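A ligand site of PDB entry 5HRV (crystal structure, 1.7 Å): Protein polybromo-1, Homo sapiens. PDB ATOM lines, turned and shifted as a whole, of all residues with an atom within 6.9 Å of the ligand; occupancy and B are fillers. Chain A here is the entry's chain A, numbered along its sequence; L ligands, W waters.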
ATOM      1  N   SER A  39     -13.365  19.847  11.461  1.00  0.00           N
ATOM      2  CA  SER A  39     -13.485  18.583  10.764  1.00  0.00           C
ATOM      3  C   SER A  39     -12.941  18.638   9.314  1.00  0.00           C
ATOM      4  O   SER A  39     -12.767  17.586   8.715  1.00  0.00           O
ATOM      5  CB  SER A  39     -14.918  18.093  10.717  1.00  0.00           C
ATOM      6  OG  SER A  39     -15.734  19.012   9.971  1.00  0.00           O
ATOM      7  N   ALA A  40     -12.685  19.843   8.796  1.00  0.00           N
ATOM      8  CA  ALA A  40     -12.345  20.025   7.382  1.00  0.00           C
ATOM      9  C   ALA A  40     -11.299  19.000   6.889  1.00  0.00           C
ATOM     10  O   ALA A  40     -11.573  18.273   5.916  1.00  0.00           O
ATOM     11  CB  ALA A  40     -11.873  21.472   7.149  1.00  0.00           C
ATOM     12  N   ILE A  41     -10.191  18.922   7.589  1.00  0.00           N
ATOM     13  CA  ILE A  41      -9.033  18.063   7.213  1.00  0.00           C
ATOM     14  C   ILE A  41      -9.365  16.567   7.348  1.00  0.00           C
ATOM     15  O   ILE A  41      -8.729  15.742   6.687  1.00  0.00           O
ATOM     16  CB  ILE A  41      -7.769  18.445   8.029  1.00  0.00           C
ATOM     17  CG1 ILE A  41      -6.491  17.929   7.403  1.00  0.00           C
ATOM     18  CG2 ILE A  41      -7.794  17.965   9.482  1.00  0.00           C
ATOM     19  CD1 ILE A  41      -6.077  18.673   6.148  1.00  0.00           C
ATOM     20  N   PHE A  42     -10.355  16.224   8.176  1.00  0.00           N
ATOM     21  CA  PHE A  42     -10.621  14.818   8.522  1.00  0.00           C
ATOM     22  C   PHE A  42     -11.642  14.169   7.619  1.00  0.00           C
ATOM     23  O   PHE A  42     -11.906  12.957   7.729  1.00  0.00           O
ATOM     24  CB  PHE A  42     -11.137  14.729   9.975  1.00  0.00           C
ATOM     25  CG  PHE A  42     -10.106  15.153  10.987  1.00  0.00           C
ATOM     26  CD1 PHE A  42      -9.068  14.326  11.293  1.00  0.00           C
ATOM     27  CD2 PHE A  42     -10.161  16.405  11.581  1.00  0.00           C
ATOM     28  CE1 PHE A  42      -8.122  14.708  12.257  1.00  0.00           C
ATOM     29  CE2 PHE A  42      -9.217  16.801  12.511  1.00  0.00           C
ATOM     30  CZ  PHE A  42      -8.182  15.934  12.867  1.00  0.00           C
ATOM     31  N   LEU A  43     -12.235  14.934   6.680  1.00  0.00           N
ATOM     32  CA  LEU A  43     -13.275  14.388   5.905  1.00  0.00           C
ATOM     33  C   LEU A  43     -12.814  13.272   4.989  1.00  0.00           C
ATOM     34  O   LEU A  43     -13.448  12.223   4.926  1.00  0.00           O
ATOM     35  CB  LEU A  43     -13.957  15.489   5.077  1.00  0.00           C
ATOM     36  CG  LEU A  43     -14.742  16.588   5.821  1.00  0.00           C
ATOM     37  CD1 LEU A  43     -15.649  17.267   4.782  1.00  0.00           C
ATOM     38  CD2 LEU A  43     -15.611  15.999   6.910  1.00  0.00           C
ATOM     39  N   ARG A  44     -11.685  13.478   4.325  1.00  0.00           N
ATOM     40  CA  ARG A  44     -11.179  12.508   3.350  1.00  0.00           C
ATOM     41  C   ARG A  44      -9.672  12.491   3.388  1.00  0.00           C
ATOM     42  O   ARG A  44      -9.013  13.484   3.166  1.00  0.00           O
ATOM     43  CB  ARG A  44     -11.677  12.880   1.950  1.00  0.00           C
ATOM     44  CG  ARG A  44     -11.360  11.873   0.885  1.00  0.00           C
ATOM     45  CD  ARG A  44     -12.253  10.640   1.007  1.00  0.00           C
ATOM     46  NE  ARG A  44     -11.949   9.659  -0.035  1.00  0.00           N
ATOM     47  CZ  ARG A  44     -11.319   8.504   0.137  1.00  0.00           C
ATOM     48  NH1 ARG A  44     -10.842   8.108   1.329  1.00  0.00           N
ATOM     49  NH2 ARG A  44     -11.147   7.719  -0.937  1.00  0.00           N
ATOM     50  N   LEU A  45      -9.124  11.326   3.704  1.00  0.00           N
ATOM     51  CA  LEU A  45      -7.721  11.111   3.625  1.00  0.00           C
ATOM     52  C   LEU A  45      -7.205  11.346   2.179  1.00  0.00           C
ATOM     53  O   LEU A  45      -7.873  10.924   1.245  1.00  0.00           O
ATOM     54  CB  LEU A  45      -7.384   9.679   3.966  1.00  0.00           C
ATOM     55  CG  LEU A  45      -7.134   9.364   5.441  1.00  0.00           C
ATOM     56  CD1 LEU A  45      -7.226   7.853   5.647  1.00  0.00           C
ATOM     57  CD2 LEU A  45      -5.781   9.880   5.885  1.00  0.00           C
ATOM     58  N   PRO A  46      -6.033  11.942   2.046  1.00  0.00           N
ATOM     59  CA  PRO A  46      -5.311  11.925   0.742  1.00  0.00           C
ATOM     60  C   PRO A  46      -4.907  10.480   0.366  1.00  0.00           C
ATOM     61  O   PRO A  46      -5.046   9.549   1.164  1.00  0.00           O
ATOM     62  CB  PRO A  46      -4.076  12.740   1.028  1.00  0.00           C
ATOM     63  CG  PRO A  46      -4.404  13.540   2.267  1.00  0.00           C
ATOM     64  CD  PRO A  46      -5.221  12.592   3.067  1.00  0.00           C
ATOM     65  N   LEU A  51       0.261  10.974   0.785  1.00  0.00           N
ATOM     66  CA  LEU A  51       0.543  10.900   2.249  1.00  0.00           C
ATOM     67  C   LEU A  51       1.173   9.534   2.588  1.00  0.00           C
ATOM     68  O   LEU A  51       0.694   8.764   3.408  1.00  0.00           O
ATOM     69  CB  LEU A  51      -0.760  11.156   3.039  1.00  0.00           C
ATOM     70  CG  LEU A  51      -0.490  11.693   4.455  1.00  0.00           C
ATOM     71  CD1 LEU A  51       0.021  13.128   4.421  1.00  0.00           C
ATOM     72  CD2 LEU A  51      -1.799  11.631   5.249  1.00  0.00           C
ATOM     73  N   TYR A  54       1.901   8.308   6.282  1.00  0.00           N
ATOM     74  CA  TYR A  54       0.725   7.935   7.008  1.00  0.00           C
ATOM     75  C   TYR A  54       0.411   6.479   6.729  1.00  0.00           C
ATOM     76  O   TYR A  54       0.269   5.665   7.634  1.00  0.00           O
ATOM     77  CB  TYR A  54      -0.482   8.868   6.666  1.00  0.00           C
ATOM     78  CG  TYR A  54      -1.808   8.445   7.262  1.00  0.00           C
ATOM     79  CD1 TYR A  54      -2.527   7.439   6.691  1.00  0.00           C
ATOM     80  CD2 TYR A  54      -2.339   9.055   8.415  1.00  0.00           C
ATOM     81  CE1 TYR A  54      -3.733   7.011   7.195  1.00  0.00           C
ATOM     82  CE2 TYR A  54      -3.559   8.635   8.945  1.00  0.00           C
ATOM     83  CZ  TYR A  54      -4.251   7.607   8.333  1.00  0.00           C
ATOM     84  OH  TYR A  54      -5.472   7.130   8.794  1.00  0.00           O
ATOM     85  N   ILE A  58       0.409   3.823   9.839  1.00  0.00           N
ATOM     86  CA  ILE A  58      -0.926   3.703  10.495  1.00  0.00           C
ATOM     87  C   ILE A  58      -1.557   2.388  10.069  1.00  0.00           C
ATOM     88  O   ILE A  58      -1.843   2.143   8.891  1.00  0.00           O
ATOM     89  CB  ILE A  58      -1.809   4.955  10.146  1.00  0.00           C
ATOM     90  CG1 ILE A  58      -1.208   6.240  10.752  1.00  0.00           C
ATOM     91  CG2 ILE A  58      -3.240   4.725  10.580  1.00  0.00           C
ATOM     92  CD1 ILE A  58      -1.095   6.275  12.283  1.00  0.00           C
ATOM     93  N   MET A  62      -8.436   5.720   8.661  1.00  0.00           N
ATOM     94  CA  MET A  62      -9.820   6.115   8.961  1.00  0.00           C
ATOM     95  C   MET A  62     -10.009   7.556   8.604  1.00  0.00           C
ATOM     96  O   MET A  62      -9.152   8.388   8.888  1.00  0.00           O
ATOM     97  CB  MET A  62     -10.097   5.901  10.448  1.00  0.00           C
ATOM     98  CG  MET A  62     -11.537   6.087  10.841  1.00  0.00           C
ATOM     99  SD  MET A  62     -12.710   4.987  10.050  1.00  0.00           S
ATOM    100  CE  MET A  62     -12.093   3.412  10.563  1.00  0.00           C
ATOM    101  N   ASP A  63     -11.156   7.874   7.985  1.00  0.00           N
ATOM    102  CA  ASP A  63     -11.558   9.253   7.738  1.00  0.00           C
ATOM    103  C   ASP A  63     -13.073   9.359   7.917  1.00  0.00           C
ATOM    104  O   ASP A  63     -13.745   8.349   8.100  1.00  0.00           O
ATOM    105  CB  ASP A  63     -11.007   9.748   6.371  1.00  0.00           C
ATOM    106  CG  ASP A  63     -11.568   9.012   5.147  1.00  0.00           C
ATOM    107  OD1 ASP A  63     -12.637   8.344   5.202  1.00  0.00           O
ATOM    108  OD2 ASP A  63     -10.925   9.162   4.091  1.00  0.00           O
ATOM    109  N   MET A  64     -13.610  10.582   7.914  1.00  0.00           N
ATOM    110  CA  MET A  64     -15.041  10.721   8.195  1.00  0.00           C
ATOM    111  C   MET A  64     -15.886  10.235   7.054  1.00  0.00           C
ATOM    112  O   MET A  64     -16.984   9.772   7.274  1.00  0.00           O
ATOM    113  CB  MET A  64     -15.393  12.147   8.564  1.00  0.00           C
ATOM    114  CG  MET A  64     -14.793  12.478   9.937  1.00  0.00           C
ATOM    115  SD  MET A  64     -15.117  14.151  10.555  1.00  0.00           S
ATOM    116  CE  MET A  64     -16.903  14.109  10.603  1.00  0.00           C
ATOM    117  N   MET A  88     -10.406   5.904  16.826  1.00  0.00           N
ATOM    118  CA  MET A  88      -9.300   5.396  15.998  1.00  0.00           C
ATOM    119  C   MET A  88      -8.757   6.546  15.118  1.00  0.00           C
ATOM    120  O   MET A  88      -7.543   6.767  15.033  1.00  0.00           O
ATOM    121  CB  MET A  88      -9.769   4.236  15.105  1.00  0.00           C
ATOM    122  CG  MET A  88      -8.698   3.647  14.217  1.00  0.00           C
ATOM    123  SD  MET A  88      -7.296   2.950  15.134  1.00  0.00           S
ATOM    124  CE  MET A  88      -8.097   1.557  15.889  1.00  0.00           C
ATOM    125  N   MET A  89      -9.662   7.272  14.476  1.00  0.00           N
ATOM    126  CA  MET A  89      -9.232   8.360  13.621  1.00  0.00           C
ATOM    127  C   MET A  89      -8.439   9.400  14.344  1.00  0.00           C
ATOM    128  O   MET A  89      -7.374   9.866  13.888  1.00  0.00           O
ATOM    129  CB  MET A  89     -10.442   9.036  12.954  1.00  0.00           C
ATOM    130  CG  MET A  89     -10.098  10.036  11.885  1.00  0.00           C
ATOM    131  SD  MET A  89     -11.580  10.799  11.177  1.00  0.00           S
ATOM    132  CE  MET A  89     -12.116  11.879  12.538  1.00  0.00           C
ATOM    133  N   PHE A  90      -8.912   9.806  15.537  1.00  0.00           N
ATOM    134  CA  PHE A  90      -8.189  10.829  16.240  1.00  0.00           C
ATOM    135  C   PHE A  90      -6.889  10.322  16.789  1.00  0.00           C
ATOM    136  O   PHE A  90      -5.917  11.044  16.828  1.00  0.00           O
ATOM    137  CB  PHE A  90      -9.077  11.408  17.375  1.00  0.00           C
ATOM    138  CG  PHE A  90     -10.335  12.045  16.876  1.00  0.00           C
ATOM    139  CD1 PHE A  90     -10.279  12.918  15.814  1.00  0.00           C
ATOM    140  CD2 PHE A  90     -11.550  11.809  17.499  1.00  0.00           C
ATOM    141  CE1 PHE A  90     -11.441  13.525  15.330  1.00  0.00           C
ATOM    142  CE2 PHE A  90     -12.712  12.416  17.015  1.00  0.00           C
ATOM    143  CZ  PHE A  90     -12.647  13.267  15.950  1.00  0.00           C
ATOM    144  N   ASN A  91      -6.858   9.066  17.238  1.00  0.00           N
ATOM    145  CA  ASN A  91      -5.579   8.506  17.722  1.00  0.00           C
ATOM    146  C   ASN A  91      -4.575   8.356  16.588  1.00  0.00           C
ATOM    147  O   ASN A  91      -3.390   8.659  16.770  1.00  0.00           O
ATOM    148  CB  ASN A  91      -5.771   7.168  18.422  1.00  0.00           C
ATOM    149  CG  ASN A  91      -4.587   6.819  19.339  1.00  0.00           C
ATOM    150  OD1 ASN A  91      -4.203   7.601  20.204  1.00  0.00           O
ATOM    151  ND2 ASN A  91      -3.990   5.700  19.098  1.00  0.00           N
ATOM    152  N   ASN A  92      -5.059   7.963  15.420  1.00  0.00           N
ATOM    153  CA  ASN A  92      -4.212   7.960  14.210  1.00  0.00           C
ATOM    154  C   ASN A  92      -3.629   9.315  13.948  1.00  0.00           C
ATOM    155  O   ASN A  92      -2.424   9.432  13.718  1.00  0.00           O
ATOM    156  CB  ASN A  92      -4.979   7.523  12.958  1.00  0.00           C
ATOM    157  CG  ASN A  92      -5.357   6.058  12.931  1.00  0.00           C
ATOM    158  OD1 ASN A  92      -4.882   5.201  13.712  1.00  0.00           O
ATOM    159  ND2 ASN A  92      -6.263   5.750  12.049  1.00  0.00           N
ATOM    160  N   ALA A  93      -4.452  10.385  13.980  1.00  0.00           N
ATOM    161  CA  ALA A  93      -3.983  11.724  13.720  1.00  0.00           C
ATOM    162  C   ALA A  93      -2.890  12.150  14.734  1.00  0.00           C
ATOM    163  O   ALA A  93      -1.911  12.779  14.357  1.00  0.00           O
ATOM    164  CB  ALA A  93      -5.130  12.699  13.746  1.00  0.00           C
ATOM    165  N   CYS A  94      -3.101  11.773  15.990  1.00  0.00           N
ATOM    166  CA  CYS A  94      -2.211  12.136  17.064  1.00  0.00           C
ATOM    167  C   CYS A  94      -0.975  11.231  17.133  1.00  0.00           C
ATOM    168  O   CYS A  94      -0.064  11.509  17.928  1.00  0.00           O
ATOM    169  CB  CYS A  94      -2.944  12.133  18.412  1.00  0.00           C
ATOM    170  SG  CYS A  94      -4.177  13.442  18.539  1.00  0.00           S
ATOM    171  N   TYR A  96       0.505  10.068  13.971  1.00  0.00           N
ATOM    172  CA  TYR A  96       1.236  10.456  12.780  1.00  0.00           C
ATOM    173  C   TYR A  96       1.776  11.867  12.893  1.00  0.00           C
ATOM    174  O   TYR A  96       2.900  12.150  12.429  1.00  0.00           O
ATOM    175  CB  TYR A  96       0.313  10.289  11.546  1.00  0.00           C
ATOM    176  CG  TYR A  96       1.003  10.772  10.292  1.00  0.00           C
ATOM    177  CD1 TYR A  96       2.181  10.190   9.873  1.00  0.00           C
ATOM    178  CD2 TYR A  96       0.466  11.806   9.529  1.00  0.00           C
ATOM    179  CE1 TYR A  96       2.830  10.680   8.724  1.00  0.00           C
ATOM    180  CE2 TYR A  96       1.101  12.268   8.385  1.00  0.00           C
ATOM    181  CZ  TYR A  96       2.275  11.703   7.992  1.00  0.00           C
ATOM    182  OH  TYR A  96       2.929  12.209   6.872  1.00  0.00           O
ATOM    183  N   ASN A  97       1.016  12.788  13.497  1.00  0.00           N
ATOM    184  CA  ASN A  97       1.387  14.173  13.626  1.00  0.00           C
ATOM    185  C   ASN A  97       1.952  14.479  15.008  1.00  0.00           C
ATOM    186  O   ASN A  97       1.617  13.803  15.959  1.00  0.00           O
ATOM    187  CB  ASN A  97       0.195  15.077  13.346  1.00  0.00           C
ATOM    188  CG  ASN A  97      -0.359  14.891  11.957  1.00  0.00           C
ATOM    189  OD1 ASN A  97       0.162  15.462  11.006  1.00  0.00           O
ATOM    190  ND2 ASN A  97      -1.379  14.071  11.818  1.00  0.00           N
ATOM    191  N   ILE A 103      -3.185  19.870  13.406  1.00  0.00           N
ATOM    192  CA  ILE A 103      -4.055  18.707  13.202  1.00  0.00           C
ATOM    193  C   ILE A 103      -4.145  17.901  14.502  1.00  0.00           C
ATOM    194  O   ILE A 103      -5.237  17.432  14.839  1.00  0.00           O
ATOM    195  CB  ILE A 103      -3.604  17.757  12.054  1.00  0.00           C
ATOM    196  CG1 ILE A 103      -3.620  18.435  10.723  1.00  0.00           C
ATOM    197  CG2 ILE A 103      -4.600  16.616  11.924  1.00  0.00           C
ATOM    198  CD1 ILE A 103      -2.963  17.647   9.585  1.00  0.00           C
HETATM  199  C1  LIG L   1      -4.662  13.273   8.198  1.00  0.00           C
HETATM  200  C2  LIG L   1      -5.968  12.817   8.146  1.00  0.00           C
HETATM  201  C3  LIG L   1      -6.898  13.199   7.101  1.00  0.00           C
HETATM  202  C4  LIG L   1      -8.221  12.707   7.065  1.00  0.00           C
HETATM  203  C5  LIG L   1      -8.655  11.806   8.062  1.00  0.00           C
HETATM  204  C6  LIG L   1      -7.781  11.414   9.077  1.00  0.00           C
HETATM  205  C7  LIG L   1      -6.438  11.880   9.102  1.00  0.00           C
HETATM  206  C8  LIG L   1      -5.529  11.490  10.145  1.00  0.00           C
HETATM  207  O1  LIG L   1      -5.815  10.685  11.010  1.00  0.00           O
HETATM  208  O2  LIG L   1      -4.262  11.961  10.197  1.00  0.00           O
HETATM  209  C9  LIG L   1      -3.841  12.823   9.249  1.00  0.00           C
HETATM  210  N1  LIG L   1      -2.668  13.374   9.190  1.00  0.00           N
HETATM  211  N2  LIG L   1      -2.632  14.226   8.067  1.00  0.00           N
HETATM  212  C10 LIG L   1      -3.853  14.165   7.515  1.00  0.00           C
HETATM  213  C11 LIG L   1      -4.155  14.971   6.225  1.00  0.00           C
HETATM  214  C12 LIG L   1      -2.868  15.659   5.777  1.00  0.00           C
HETATM  215  O   HOH W   1      -7.387  15.342   4.380  1.00  0.00           O
HETATM  216  O   HOH W   2      -7.036   8.245  10.475  1.00  0.00           O
HETATM  217  O   HOH W   3      -0.230  15.599   8.228  1.00  0.00           O
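Water W3 bridges a nitrogen (N2) of the ligand (2.8 Å) and the side-chain amide oxygen of Asn 97 (2.8 Å).
Water W2 lies within hydrogen-bond range of OH of Tyr 54, O of Met 62, O1 of the ligand and ND2 of Asn 92.
O of Phe 42 is in hydrogen-bond range of N of Met 64, 2.9 Å away.
The side-chain carboxylate of Asp 63 sits at hydrogen-bond distance from the backbone NH of Leu 45 (2.8 Å).
OD1 of Asn 92 sits close to O of Met 88 (3.4 Å).
ND2 of Asn 97 lies within hydrogen-bond range of O of Ala 93, 2.9 Å away.
The side-chain carboxylate (OD2) of Asp 63 is in salt-bridge range of the guanidinium group (NH1) of Arg 44 (3.0 Å).
N of Met 62 is in hydrogen-bond range of OH of Tyr 54 (3.3 Å).
The backbone NH (N) of Ala 93 sits at hydrogen-bond distance from an oxygen (O1) of the ligand, at 3.3 Å.
ND2 of Asn 97 sits close to N1 of the ligand (3.0 Å).
The backbone carbonyl oxygen (O) of Met 89 sits close to an oxygen (O1) of the ligand (3.4 Å).
Ile 41 touches the ligand (O to C4, 3.1 Å).
Phe 42 touches the ligand (O to C5, 3.5 Å).
Arg 44 touches the ligand (C to C4, 3.96 Å).
CD2 of Leu 45 touches C3 of the ligand, at 3.7 Å.
Leu 51 touches the ligand (CD2 to N2, 3.9 Å).
Tyr 54 touches the ligand (CE2 to O2, 3.6 Å).
O of Met 62 touches C6 of the ligand, 3.3 Å away.
Asp 63 touches the ligand (CB to C5, 3.6 Å).
Asn 92 touches the ligand.
Tyr 96 touches the ligand (CD2 to N1, 3.5 Å).
CD1 of Ile 103 touches N2 of the ligand, at 3.8 Å.
Of the 24 residues printed, 14 come within 4 Å of the ligand.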
